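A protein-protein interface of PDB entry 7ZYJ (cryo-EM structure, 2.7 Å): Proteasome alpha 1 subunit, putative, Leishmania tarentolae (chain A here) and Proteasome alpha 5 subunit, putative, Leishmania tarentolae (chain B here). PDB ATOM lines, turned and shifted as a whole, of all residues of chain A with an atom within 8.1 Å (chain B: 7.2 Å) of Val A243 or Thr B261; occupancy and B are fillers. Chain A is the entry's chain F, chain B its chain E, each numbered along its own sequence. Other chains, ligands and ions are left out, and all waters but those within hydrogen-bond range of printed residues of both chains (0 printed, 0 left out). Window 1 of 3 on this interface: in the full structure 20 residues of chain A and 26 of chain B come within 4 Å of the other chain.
The side-chain hydroxyl (OG1) of Thr B263 is in hydrogen-bond range of the side-chain amide nitrogen (NE2) of Gln A225 (2.5 Å).
The side-chain amide oxygen (OE1) of Gln A225 lies within hydrogen-bond range of the side-chain amino group (NZ) of Lys A227 (3.4 Å).
O of Thr B213 is in hydrogen-bond range of SG of Cys B217, 3.1 Å away.
OG1 of Thr B261 is in hydrogen-bond range of OG of Ser B259 (3.2 Å).
The backbone carbonyl oxygen (O) of Thr B263 sits at hydrogen-bond distance from the backbone NH (N) of Gln B255.
O of Tyr A224 touches CG2 of Thr B263, at 3.3 Å.
Thr B261 touches Gln A225 (CG2 to NE2, 3.3 Å).
CG of Gln A225 touches O of His B262 (3.9 Å).
Thr B261 touches Val A243 (CG2 to CB, 3.7 Å).
Ala A244 touches Ser B259.
Arg A247 touches Cys B217 (NH1 to CB, 3.9 Å).
Arg A247 touches Gly B260 (NH1 to O, 3.7 Å).
His B262 touches Arg A247.
Val A248 touches Ile B221 (CG2 to CD1, 3.9 Å).
Gly B260 touches just one residue of chain A: Arg A247 (3.7 Å).
Printed residues of chain B within 4 Å of Arg A247: Cys B217 (3.9 Å), Gly B260 (3.7 Å) and His B262 (3.97 Å).
Of the printed residues of chain A, Cys B217 touches Arg A247.
Printed residues of chain B within 4 Å of Gln A225: Thr B261 (3.3 Å), His B262 (3.9 Å) and Thr B263 (2.5 Å).
Of the printed residues of chain A, Ser B259 touches Ala A244.
Ser A197 touches none of the printed residues of chain B.
Asp B257 touches none of the printed residues of chain A.
The nearest printed residue of chain B that does not touch Gln A225 is Asp B257 (5.8 Å).
Hydrophobic or aromatic side chains of chain B that line the printed part of chain A: Ile B221 and His B262.
Hydrophobic or aromatic side chains of chain A within 4 Å of the printed part of chain B: Val A243, Ala A244 and Val A248.
Among the printed residues, 10 pairs touch across the chains.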
ATOM      1  N   SER A 197     -36.597 -14.962  -4.710  1.00  0.00           N
ATOM      2  CA  SER A 197     -37.311 -14.689  -5.949  1.00  0.00           C
ATOM      3  C   SER A 197     -37.978 -15.955  -6.472  1.00  0.00           C
ATOM      4  O   SER A 197     -37.430 -17.055  -6.370  1.00  0.00           O
ATOM      5  CB  SER A 197     -36.357 -14.125  -7.001  1.00  0.00           C
ATOM      6  OG  SER A 197     -35.526 -15.140  -7.535  1.00  0.00           O
ATOM      7  N   TYR A 224     -28.598  -6.340 -11.898  1.00  0.00           N
ATOM      8  CA  TYR A 224     -28.469  -7.705 -12.380  1.00  0.00           C
ATOM      9  C   TYR A 224     -27.838  -8.578 -11.307  1.00  0.00           C
ATOM     10  O   TYR A 224     -26.844  -8.194 -10.683  1.00  0.00           O
ATOM     11  CB  TYR A 224     -27.632  -7.769 -13.659  1.00  0.00           C
ATOM     12  CG  TYR A 224     -27.211  -9.171 -14.033  1.00  0.00           C
ATOM     13  CD1 TYR A 224     -28.103 -10.043 -14.642  1.00  0.00           C
ATOM     14  CD2 TYR A 224     -25.924  -9.625 -13.776  1.00  0.00           C
ATOM     15  CE1 TYR A 224     -27.725 -11.327 -14.984  1.00  0.00           C
ATOM     16  CE2 TYR A 224     -25.538 -10.905 -14.113  1.00  0.00           C
ATOM     17  CZ  TYR A 224     -26.442 -11.752 -14.718  1.00  0.00           C
ATOM     18  OH  TYR A 224     -26.059 -13.028 -15.056  1.00  0.00           O
ATOM     19  N   GLN A 225     -28.422  -9.755 -11.099  1.00  0.00           N
ATOM     20  CA  GLN A 225     -27.903 -10.734 -10.158  1.00  0.00           C
ATOM     21  C   GLN A 225     -28.104 -12.118 -10.755  1.00  0.00           C
ATOM     22  O   GLN A 225     -29.215 -12.457 -11.171  1.00  0.00           O
ATOM     23  CB  GLN A 225     -28.605 -10.625  -8.802  1.00  0.00           C
ATOM     24  CG  GLN A 225     -27.843 -11.242  -7.648  1.00  0.00           C
ATOM     25  CD  GLN A 225     -28.413 -10.836  -6.307  1.00  0.00           C
ATOM     26  OE1 GLN A 225     -29.315 -11.487  -5.780  1.00  0.00           O
ATOM     27  NE2 GLN A 225     -27.897  -9.749  -5.749  1.00  0.00           N
ATOM     28  N   GLU A 226     -27.035 -12.908 -10.796  1.00  0.00           N
ATOM     29  CA  GLU A 226     -27.076 -14.206 -11.456  1.00  0.00           C
ATOM     30  C   GLU A 226     -27.768 -15.223 -10.556  1.00  0.00           C
ATOM     31  O   GLU A 226     -27.279 -15.529  -9.464  1.00  0.00           O
ATOM     32  CB  GLU A 226     -25.667 -14.671 -11.810  1.00  0.00           C
ATOM     33  CG  GLU A 226     -25.590 -16.115 -12.281  1.00  0.00           C
ATOM     34  CD  GLU A 226     -24.221 -16.479 -12.818  1.00  0.00           C
ATOM     35  OE1 GLU A 226     -24.146 -17.318 -13.740  1.00  0.00           O
ATOM     36  OE2 GLU A 226     -23.219 -15.927 -12.317  1.00  0.00           O
ATOM     37  N   LYS A 227     -28.903 -15.743 -11.016  1.00  0.00           N
ATOM     38  CA  LYS A 227     -29.655 -16.768 -10.302  1.00  0.00           C
ATOM     39  C   LYS A 227     -29.612 -18.125 -10.983  1.00  0.00           C
ATOM     40  O   LYS A 227     -29.566 -19.150 -10.300  1.00  0.00           O
ATOM     41  CB  LYS A 227     -31.116 -16.334 -10.142  1.00  0.00           C
ATOM     42  CG  LYS A 227     -31.290 -14.973  -9.490  1.00  0.00           C
ATOM     43  CD  LYS A 227     -30.769 -14.972  -8.065  1.00  0.00           C
ATOM     44  CE  LYS A 227     -31.651 -14.133  -7.158  1.00  0.00           C
ATOM     45  NZ  LYS A 227     -31.801 -12.741  -7.665  1.00  0.00           N
ATOM     46  N   PHE A 229     -27.683 -20.912 -13.167  1.00  0.00           N
ATOM     47  CA  PHE A 229     -26.315 -21.327 -13.424  1.00  0.00           C
ATOM     48  C   PHE A 229     -26.306 -22.523 -14.362  1.00  0.00           C
ATOM     49  O   PHE A 229     -27.232 -23.339 -14.366  1.00  0.00           O
ATOM     50  CB  PHE A 229     -25.579 -21.689 -12.126  1.00  0.00           C
ATOM     51  CG  PHE A 229     -25.459 -20.551 -11.156  1.00  0.00           C
ATOM     52  CD1 PHE A 229     -26.519 -20.207 -10.335  1.00  0.00           C
ATOM     53  CD2 PHE A 229     -24.283 -19.828 -11.062  1.00  0.00           C
ATOM     54  CE1 PHE A 229     -26.410 -19.162  -9.442  1.00  0.00           C
ATOM     55  CE2 PHE A 229     -24.168 -18.782 -10.169  1.00  0.00           C
ATOM     56  CZ  PHE A 229     -25.232 -18.449  -9.358  1.00  0.00           C
ATOM     57  N   MET A 237     -29.183 -25.214 -13.291  1.00  0.00           N
ATOM     58  CA  MET A 237     -30.010 -25.089 -12.100  1.00  0.00           C
ATOM     59  C   MET A 237     -30.417 -23.641 -11.875  1.00  0.00           C
ATOM     60  O   MET A 237     -29.802 -22.718 -12.411  1.00  0.00           O
ATOM     61  CB  MET A 237     -29.287 -25.626 -10.861  1.00  0.00           C
ATOM     62  CG  MET A 237     -28.298 -24.663 -10.246  1.00  0.00           C
ATOM     63  SD  MET A 237     -27.516 -25.365  -8.787  1.00  0.00           S
ATOM     64  CE  MET A 237     -26.477 -24.001  -8.291  1.00  0.00           C
ATOM     65  N   ILE A 239     -31.456 -21.016  -8.598  1.00  0.00           N
ATOM     66  CA  ILE A 239     -31.329 -20.872  -7.158  1.00  0.00           C
ATOM     67  C   ILE A 239     -32.444 -19.972  -6.643  1.00  0.00           C
ATOM     68  O   ILE A 239     -33.036 -19.179  -7.381  1.00  0.00           O
ATOM     69  CB  ILE A 239     -29.944 -20.316  -6.758  1.00  0.00           C
ATOM     70  CG1 ILE A 239     -29.861 -18.819  -7.054  1.00  0.00           C
ATOM     71  CG2 ILE A 239     -28.844 -21.042  -7.506  1.00  0.00           C
ATOM     72  CD1 ILE A 239     -28.635 -18.151  -6.472  1.00  0.00           C
ATOM     73  N   SER A 240     -32.745 -20.105  -5.353  1.00  0.00           N
ATOM     74  CA  SER A 240     -33.686 -19.209  -4.692  1.00  0.00           C
ATOM     75  C   SER A 240     -33.320 -19.107  -3.220  1.00  0.00           C
ATOM     76  O   SER A 240     -33.276 -20.121  -2.522  1.00  0.00           O
ATOM     77  CB  SER A 240     -35.129 -19.700  -4.848  1.00  0.00           C
ATOM     78  OG  SER A 240     -36.008 -18.983  -4.000  1.00  0.00           O
ATOM     79  N   GLY A 241     -33.073 -17.888  -2.750  1.00  0.00           N
ATOM     80  CA  GLY A 241     -32.699 -17.688  -1.364  1.00  0.00           C
ATOM     81  C   GLY A 241     -31.380 -16.964  -1.200  1.00  0.00           C
ATOM     82  O   GLY A 241     -31.180 -15.890  -1.774  1.00  0.00           O
ATOM     83  N   LEU A 242     -30.471 -17.541  -0.420  1.00  0.00           N
ATOM     84  CA  LEU A 242     -29.159 -16.942  -0.193  1.00  0.00           C
ATOM     85  C   LEU A 242     -28.303 -17.150  -1.437  1.00  0.00           C
ATOM     86  O   LEU A 242     -28.006 -18.287  -1.813  1.00  0.00           O
ATOM     87  CB  LEU A 242     -28.499 -17.548   1.042  1.00  0.00           C
ATOM     88  CG  LEU A 242     -29.181 -17.259   2.380  1.00  0.00           C
ATOM     89  CD1 LEU A 242     -28.315 -17.732   3.535  1.00  0.00           C
ATOM     90  CD2 LEU A 242     -29.497 -15.778   2.515  1.00  0.00           C
ATOM     91  N   VAL A 243     -27.910 -16.046  -2.076  1.00  0.00           N
ATOM     92  CA  VAL A 243     -27.163 -16.129  -3.327  1.00  0.00           C
ATOM     93  C   VAL A 243     -25.774 -16.712  -3.106  1.00  0.00           C
ATOM     94  O   VAL A 243     -25.255 -17.433  -3.965  1.00  0.00           O
ATOM     95  CB  VAL A 243     -27.094 -14.742  -3.994  1.00  0.00           C
ATOM     96  CG1 VAL A 243     -26.570 -14.860  -5.414  1.00  0.00           C
ATOM     97  CG2 VAL A 243     -28.462 -14.085  -3.981  1.00  0.00           C
ATOM     98  N   ALA A 244     -25.140 -16.402  -1.972  1.00  0.00           N
ATOM     99  CA  ALA A 244     -23.814 -16.946  -1.698  1.00  0.00           C
ATOM    100  C   ALA A 244     -23.847 -18.463  -1.556  1.00  0.00           C
ATOM    101  O   ALA A 244     -22.955 -19.156  -2.065  1.00  0.00           O
ATOM    102  CB  ALA A 244     -23.233 -16.306  -0.438  1.00  0.00           C
ATOM    103  N   ASP A 245     -24.861 -18.994  -0.871  1.00  0.00           N
ATOM    104  CA  ASP A 245     -25.017 -20.440  -0.771  1.00  0.00           C
ATOM    105  C   ASP A 245     -25.253 -21.064  -2.140  1.00  0.00           C
ATOM    106  O   ASP A 245     -24.714 -22.137  -2.439  1.00  0.00           O
ATOM    107  CB  ASP A 245     -26.167 -20.776   0.178  1.00  0.00           C
ATOM    108  CG  ASP A 245     -25.849 -20.442   1.620  1.00  0.00           C
ATOM    109  OD1 ASP A 245     -24.740 -19.933   1.883  1.00  0.00           O
ATOM    110  OD2 ASP A 245     -26.709 -20.686   2.491  1.00  0.00           O
ATOM    111  N   GLY A 246     -26.055 -20.407  -2.979  1.00  0.00           N
ATOM    112  CA  GLY A 246     -26.239 -20.880  -4.339  1.00  0.00           C
ATOM    113  C   GLY A 246     -24.952 -20.897  -5.137  1.00  0.00           C
ATOM    114  O   GLY A 246     -24.713 -21.824  -5.911  1.00  0.00           O
ATOM    115  N   ARG A 247     -24.106 -19.881  -4.958  1.00  0.00           N
ATOM    116  CA  ARG A 247     -22.816 -19.858  -5.642  1.00  0.00           C
ATOM    117  C   ARG A 247     -21.914 -20.988  -5.162  1.00  0.00           C
ATOM    118  O   ARG A 247     -21.228 -21.628  -5.969  1.00  0.00           O
ATOM    119  CB  ARG A 247     -22.135 -18.507  -5.431  1.00  0.00           C
ATOM    120  CG  ARG A 247     -22.659 -17.398  -6.321  1.00  0.00           C
ATOM    121  CD  ARG A 247     -21.868 -16.121  -6.114  1.00  0.00           C
ATOM    122  NE  ARG A 247     -20.451 -16.307  -6.404  1.00  0.00           N
ATOM    123  CZ  ARG A 247     -19.470 -16.017  -5.561  1.00  0.00           C
ATOM    124  NH1 ARG A 247     -19.715 -15.522  -4.359  1.00  0.00           N
ATOM    125  NH2 ARG A 247     -18.210 -16.229  -5.933  1.00  0.00           N
ATOM    126  N   VAL A 248     -21.894 -21.241  -3.852  1.00  0.00           N
ATOM    127  CA  VAL A 248     -21.091 -22.341  -3.321  1.00  0.00           C
ATOM    128  C   VAL A 248     -21.573 -23.672  -3.885  1.00  0.00           C
ATOM    129  O   VAL A 248     -20.770 -24.522  -4.298  1.00  0.00           O
ATOM    130  CB  VAL A 248     -21.126 -22.332  -1.781  1.00  0.00           C
ATOM    131  CG1 VAL A 248     -20.444 -23.570  -1.225  1.00  0.00           C
ATOM    132  CG2 VAL A 248     -20.466 -21.073  -1.245  1.00  0.00           C
ATOM    133  N   LEU A 249     -22.892 -23.871  -3.918  1.00  0.00           N
ATOM    134  CA  LEU A 249     -23.442 -25.112  -4.453  1.00  0.00           C
ATOM    135  C   LEU A 249     -23.162 -25.246  -5.944  1.00  0.00           C
ATOM    136  O   LEU A 249     -22.894 -26.349  -6.431  1.00  0.00           O
ATOM    137  CB  LEU A 249     -24.941 -25.178  -4.167  1.00  0.00           C
ATOM    138  CG  LEU A 249     -25.276 -25.376  -2.687  1.00  0.00           C
ATOM    139  CD1 LEU A 249     -26.765 -25.563  -2.480  1.00  0.00           C
ATOM    140  CD2 LEU A 249     -24.504 -26.555  -2.120  1.00  0.00           C
ATOM    141  N   ALA A 250     -23.217 -24.136  -6.685  1.00  0.00           N
ATOM    142  CA  ALA A 250     -22.878 -24.169  -8.103  1.00  0.00           C
ATOM    143  C   ALA A 250     -21.423 -24.560  -8.313  1.00  0.00           C
ATOM    144  O   ALA A 250     -21.111 -25.361  -9.200  1.00  0.00           O
ATOM    145  CB  ALA A 250     -23.160 -22.811  -8.744  1.00  0.00           C
ATOM    146  N   GLY A 294     -28.976 -21.783   3.130  1.00  0.00           N
ATOM    147  CA  GLY A 294     -30.222 -21.045   3.068  1.00  0.00           C
ATOM    148  C   GLY A 294     -30.691 -20.801   1.649  1.00  0.00           C
ATOM    149  O   GLY A 294     -31.131 -19.698   1.314  1.00  0.00           O
ATOM    150  N   VAL A 295     -30.608 -21.827   0.809  1.00  0.00           N
ATOM    151  CA  VAL A 295     -30.963 -21.705  -0.600  1.00  0.00           C
ATOM    152  C   VAL A 295     -31.646 -22.991  -1.042  1.00  0.00           C
ATOM    153  O   VAL A 295     -31.330 -24.081  -0.555  1.00  0.00           O
ATOM    154  CB  VAL A 295     -29.720 -21.390  -1.464  1.00  0.00           C
ATOM    155  CG1 VAL A 295     -28.794 -22.593  -1.543  1.00  0.00           C
ATOM    156  CG2 VAL A 295     -30.131 -20.932  -2.855  1.00  0.00           C
ATOM    157  N   THR B 213     -14.960  -8.763  -8.606  1.00  0.00           N
ATOM    158  CA  THR B 213     -15.994  -8.762  -7.579  1.00  0.00           C
ATOM    159  C   THR B 213     -16.263 -10.175  -7.075  1.00  0.00           C
ATOM    160  O   THR B 213     -16.508 -10.382  -5.881  1.00  0.00           O
ATOM    161  CB  THR B 213     -17.272  -8.127  -8.126  1.00  0.00           C
ATOM    162  OG1 THR B 213     -16.935  -6.965  -8.892  1.00  0.00           O
ATOM    163  CG2 THR B 213     -18.178  -7.710  -6.987  1.00  0.00           C
ATOM    164  N   CYS B 217     -15.975 -11.322  -3.174  1.00  0.00           N
ATOM    165  CA  CYS B 217     -17.033 -12.004  -2.434  1.00  0.00           C
ATOM    166  C   CYS B 217     -16.606 -13.398  -1.991  1.00  0.00           C
ATOM    167  O   CYS B 217     -17.037 -13.869  -0.933  1.00  0.00           O
ATOM    168  CB  CYS B 217     -18.307 -12.080  -3.275  1.00  0.00           C
ATOM    169  SG  CYS B 217     -18.888 -10.486  -3.897  1.00  0.00           S
ATOM    170  N   SER B 220     -14.879 -12.820   1.044  1.00  0.00           N
ATOM    171  CA  SER B 220     -15.782 -12.334   2.084  1.00  0.00           C
ATOM    172  C   SER B 220     -16.579 -13.459   2.734  1.00  0.00           C
ATOM    173  O   SER B 220     -16.769 -13.454   3.955  1.00  0.00           O
ATOM    174  CB  SER B 220     -16.730 -11.286   1.501  1.00  0.00           C
ATOM    175  OG  SER B 220     -17.605 -10.782   2.494  1.00  0.00           O
ATOM    176  N   ILE B 221     -17.057 -14.423   1.944  1.00  0.00           N
ATOM    177  CA  ILE B 221     -17.955 -15.444   2.482  1.00  0.00           C
ATOM    178  C   ILE B 221     -17.271 -16.372   3.482  1.00  0.00           C
ATOM    179  O   ILE B 221     -17.958 -17.056   4.249  1.00  0.00           O
ATOM    180  CB  ILE B 221     -18.585 -16.284   1.353  1.00  0.00           C
ATOM    181  CG1 ILE B 221     -17.511 -17.086   0.615  1.00  0.00           C
ATOM    182  CG2 ILE B 221     -19.391 -15.408   0.407  1.00  0.00           C
ATOM    183  CD1 ILE B 221     -18.067 -18.104  -0.353  1.00  0.00           C
ATOM    184  N   GLN B 255     -21.620  -3.935  -6.959  1.00  0.00           N
ATOM    185  CA  GLN B 255     -21.748  -3.659  -5.539  1.00  0.00           C
ATOM    186  C   GLN B 255     -21.595  -4.960  -4.768  1.00  0.00           C
ATOM    187  O   GLN B 255     -22.126  -6.000  -5.173  1.00  0.00           O
ATOM    188  CB  GLN B 255     -23.098  -2.996  -5.226  1.00  0.00           C
ATOM    189  CG  GLN B 255     -23.251  -2.491  -3.799  1.00  0.00           C
ATOM    190  CD  GLN B 255     -23.730  -3.561  -2.844  1.00  0.00           C
ATOM    191  OE1 GLN B 255     -24.446  -4.483  -3.236  1.00  0.00           O
ATOM    192  NE2 GLN B 255     -23.339  -3.445  -1.581  1.00  0.00           N
ATOM    193  N   THR B 256     -20.864  -4.890  -3.659  1.00  0.00           N
ATOM    194  CA  THR B 256     -20.549  -6.040  -2.825  1.00  0.00           C
ATOM    195  C   THR B 256     -21.184  -5.860  -1.454  1.00  0.00           C
ATOM    196  O   THR B 256     -21.166  -4.760  -0.893  1.00  0.00           O
ATOM    197  CB  THR B 256     -19.029  -6.216  -2.686  1.00  0.00           C
ATOM    198  OG1 THR B 256     -18.466  -6.553  -3.959  1.00  0.00           O
ATOM    199  CG2 THR B 256     -18.693  -7.315  -1.691  1.00  0.00           C
ATOM    200  N   ASP B 257     -21.749  -6.935  -0.924  1.00  0.00           N
ATOM    201  CA  ASP B 257     -22.398  -6.937   0.375  1.00  0.00           C
ATOM    202  C   ASP B 257     -21.620  -7.787   1.370  1.00  0.00           C
ATOM    203  O   ASP B 257     -20.843  -8.667   0.980  1.00  0.00           O
ATOM    204  CB  ASP B 257     -23.833  -7.470   0.259  1.00  0.00           C
ATOM    205  CG  ASP B 257     -24.745  -6.524  -0.493  1.00  0.00           C
ATOM    206  OD1 ASP B 257     -24.501  -5.302  -0.449  1.00  0.00           O
ATOM    207  OD2 ASP B 257     -25.708  -7.004  -1.129  1.00  0.00           O
ATOM    208  N   PRO B 258     -21.795  -7.546   2.673  1.00  0.00           N
ATOM    209  CA  PRO B 258     -21.165  -8.422   3.674  1.00  0.00           C
ATOM    210  C   PRO B 258     -21.644  -9.861   3.607  1.00  0.00           C
ATOM    211  O   PRO B 258     -20.957 -10.747   4.130  1.00  0.00           O
ATOM    212  CB  PRO B 258     -21.551  -7.770   5.010  1.00  0.00           C
ATOM    213  CG  PRO B 258     -22.700  -6.869   4.693  1.00  0.00           C
ATOM    214  CD  PRO B 258     -22.473  -6.397   3.295  1.00  0.00           C
ATOM    215  N   SER B 259     -22.798 -10.122   2.988  1.00  0.00           N
ATOM    216  CA  SER B 259     -23.259 -11.492   2.805  1.00  0.00           C
ATOM    217  C   SER B 259     -22.487 -12.220   1.715  1.00  0.00           C
ATOM    218  O   SER B 259     -22.679 -13.427   1.539  1.00  0.00           O
ATOM    219  CB  SER B 259     -24.751 -11.505   2.477  1.00  0.00           C
ATOM    220  OG  SER B 259     -25.013 -10.827   1.263  1.00  0.00           O
ATOM    221  N   GLY B 260     -21.625 -11.520   0.983  1.00  0.00           N
ATOM    222  CA  GLY B 260     -20.912 -12.120  -0.125  1.00  0.00           C
ATOM    223  C   GLY B 260     -21.671 -12.142  -1.429  1.00  0.00           C
ATOM    224  O   GLY B 260     -21.367 -12.974  -2.291  1.00  0.00           O
ATOM    225  N   THR B 261     -22.647 -11.257  -1.603  1.00  0.00           N
ATOM    226  CA  THR B 261     -23.498 -11.228  -2.788  1.00  0.00           C
ATOM    227  C   THR B 261     -23.108 -10.027  -3.641  1.00  0.00           C
ATOM    228  O   THR B 261     -23.187  -8.882  -3.185  1.00  0.00           O
ATOM    229  CB  THR B 261     -24.972 -11.164  -2.396  1.00  0.00           C
ATOM    230  OG1 THR B 261     -25.284 -12.261  -1.529  1.00  0.00           O
ATOM    231  CG2 THR B 261     -25.850 -11.239  -3.632  1.00  0.00           C
ATOM    232  N   HIS B 262     -22.694 -10.291  -4.876  1.00  0.00           N
ATOM    233  CA  HIS B 262     -22.335  -9.242  -5.817  1.00  0.00           C
ATOM    234  C   HIS B 262     -23.517  -8.929  -6.722  1.00  0.00           C
ATOM    235  O   HIS B 262     -24.261  -9.827  -7.125  1.00  0.00           O
ATOM    236  CB  HIS B 262     -21.131  -9.667  -6.657  1.00  0.00           C
ATOM    237  CG  HIS B 262     -21.385 -10.870  -7.508  1.00  0.00           C
ATOM    238  ND1 HIS B 262     -21.853 -10.781  -8.801  1.00  0.00           N
ATOM    239  CD2 HIS B 262     -21.250 -12.192  -7.247  1.00  0.00           C
ATOM    240  CE1 HIS B 262     -21.988 -11.995  -9.303  1.00  0.00           C
ATOM    241  NE2 HIS B 262     -21.631 -12.869  -8.380  1.00  0.00           N
ATOM    242  N   THR B 263     -23.688  -7.648  -7.040  1.00  0.00           N
ATOM    243  CA  THR B 263     -24.803  -7.225  -7.879  1.00  0.00           C
ATOM    244  C   THR B 263     -24.350  -6.127  -8.828  1.00  0.00           C
ATOM    245  O   THR B 263     -23.801  -5.115  -8.388  1.00  0.00           O
ATOM    246  CB  THR B 263     -25.978  -6.729  -7.030  1.00  0.00           C
ATOM    247  OG1 THR B 263     -26.378  -7.757  -6.117  1.00  0.00           O
ATOM    248  CG2 THR B 263     -27.157  -6.361  -7.917  1.00  0.00           C
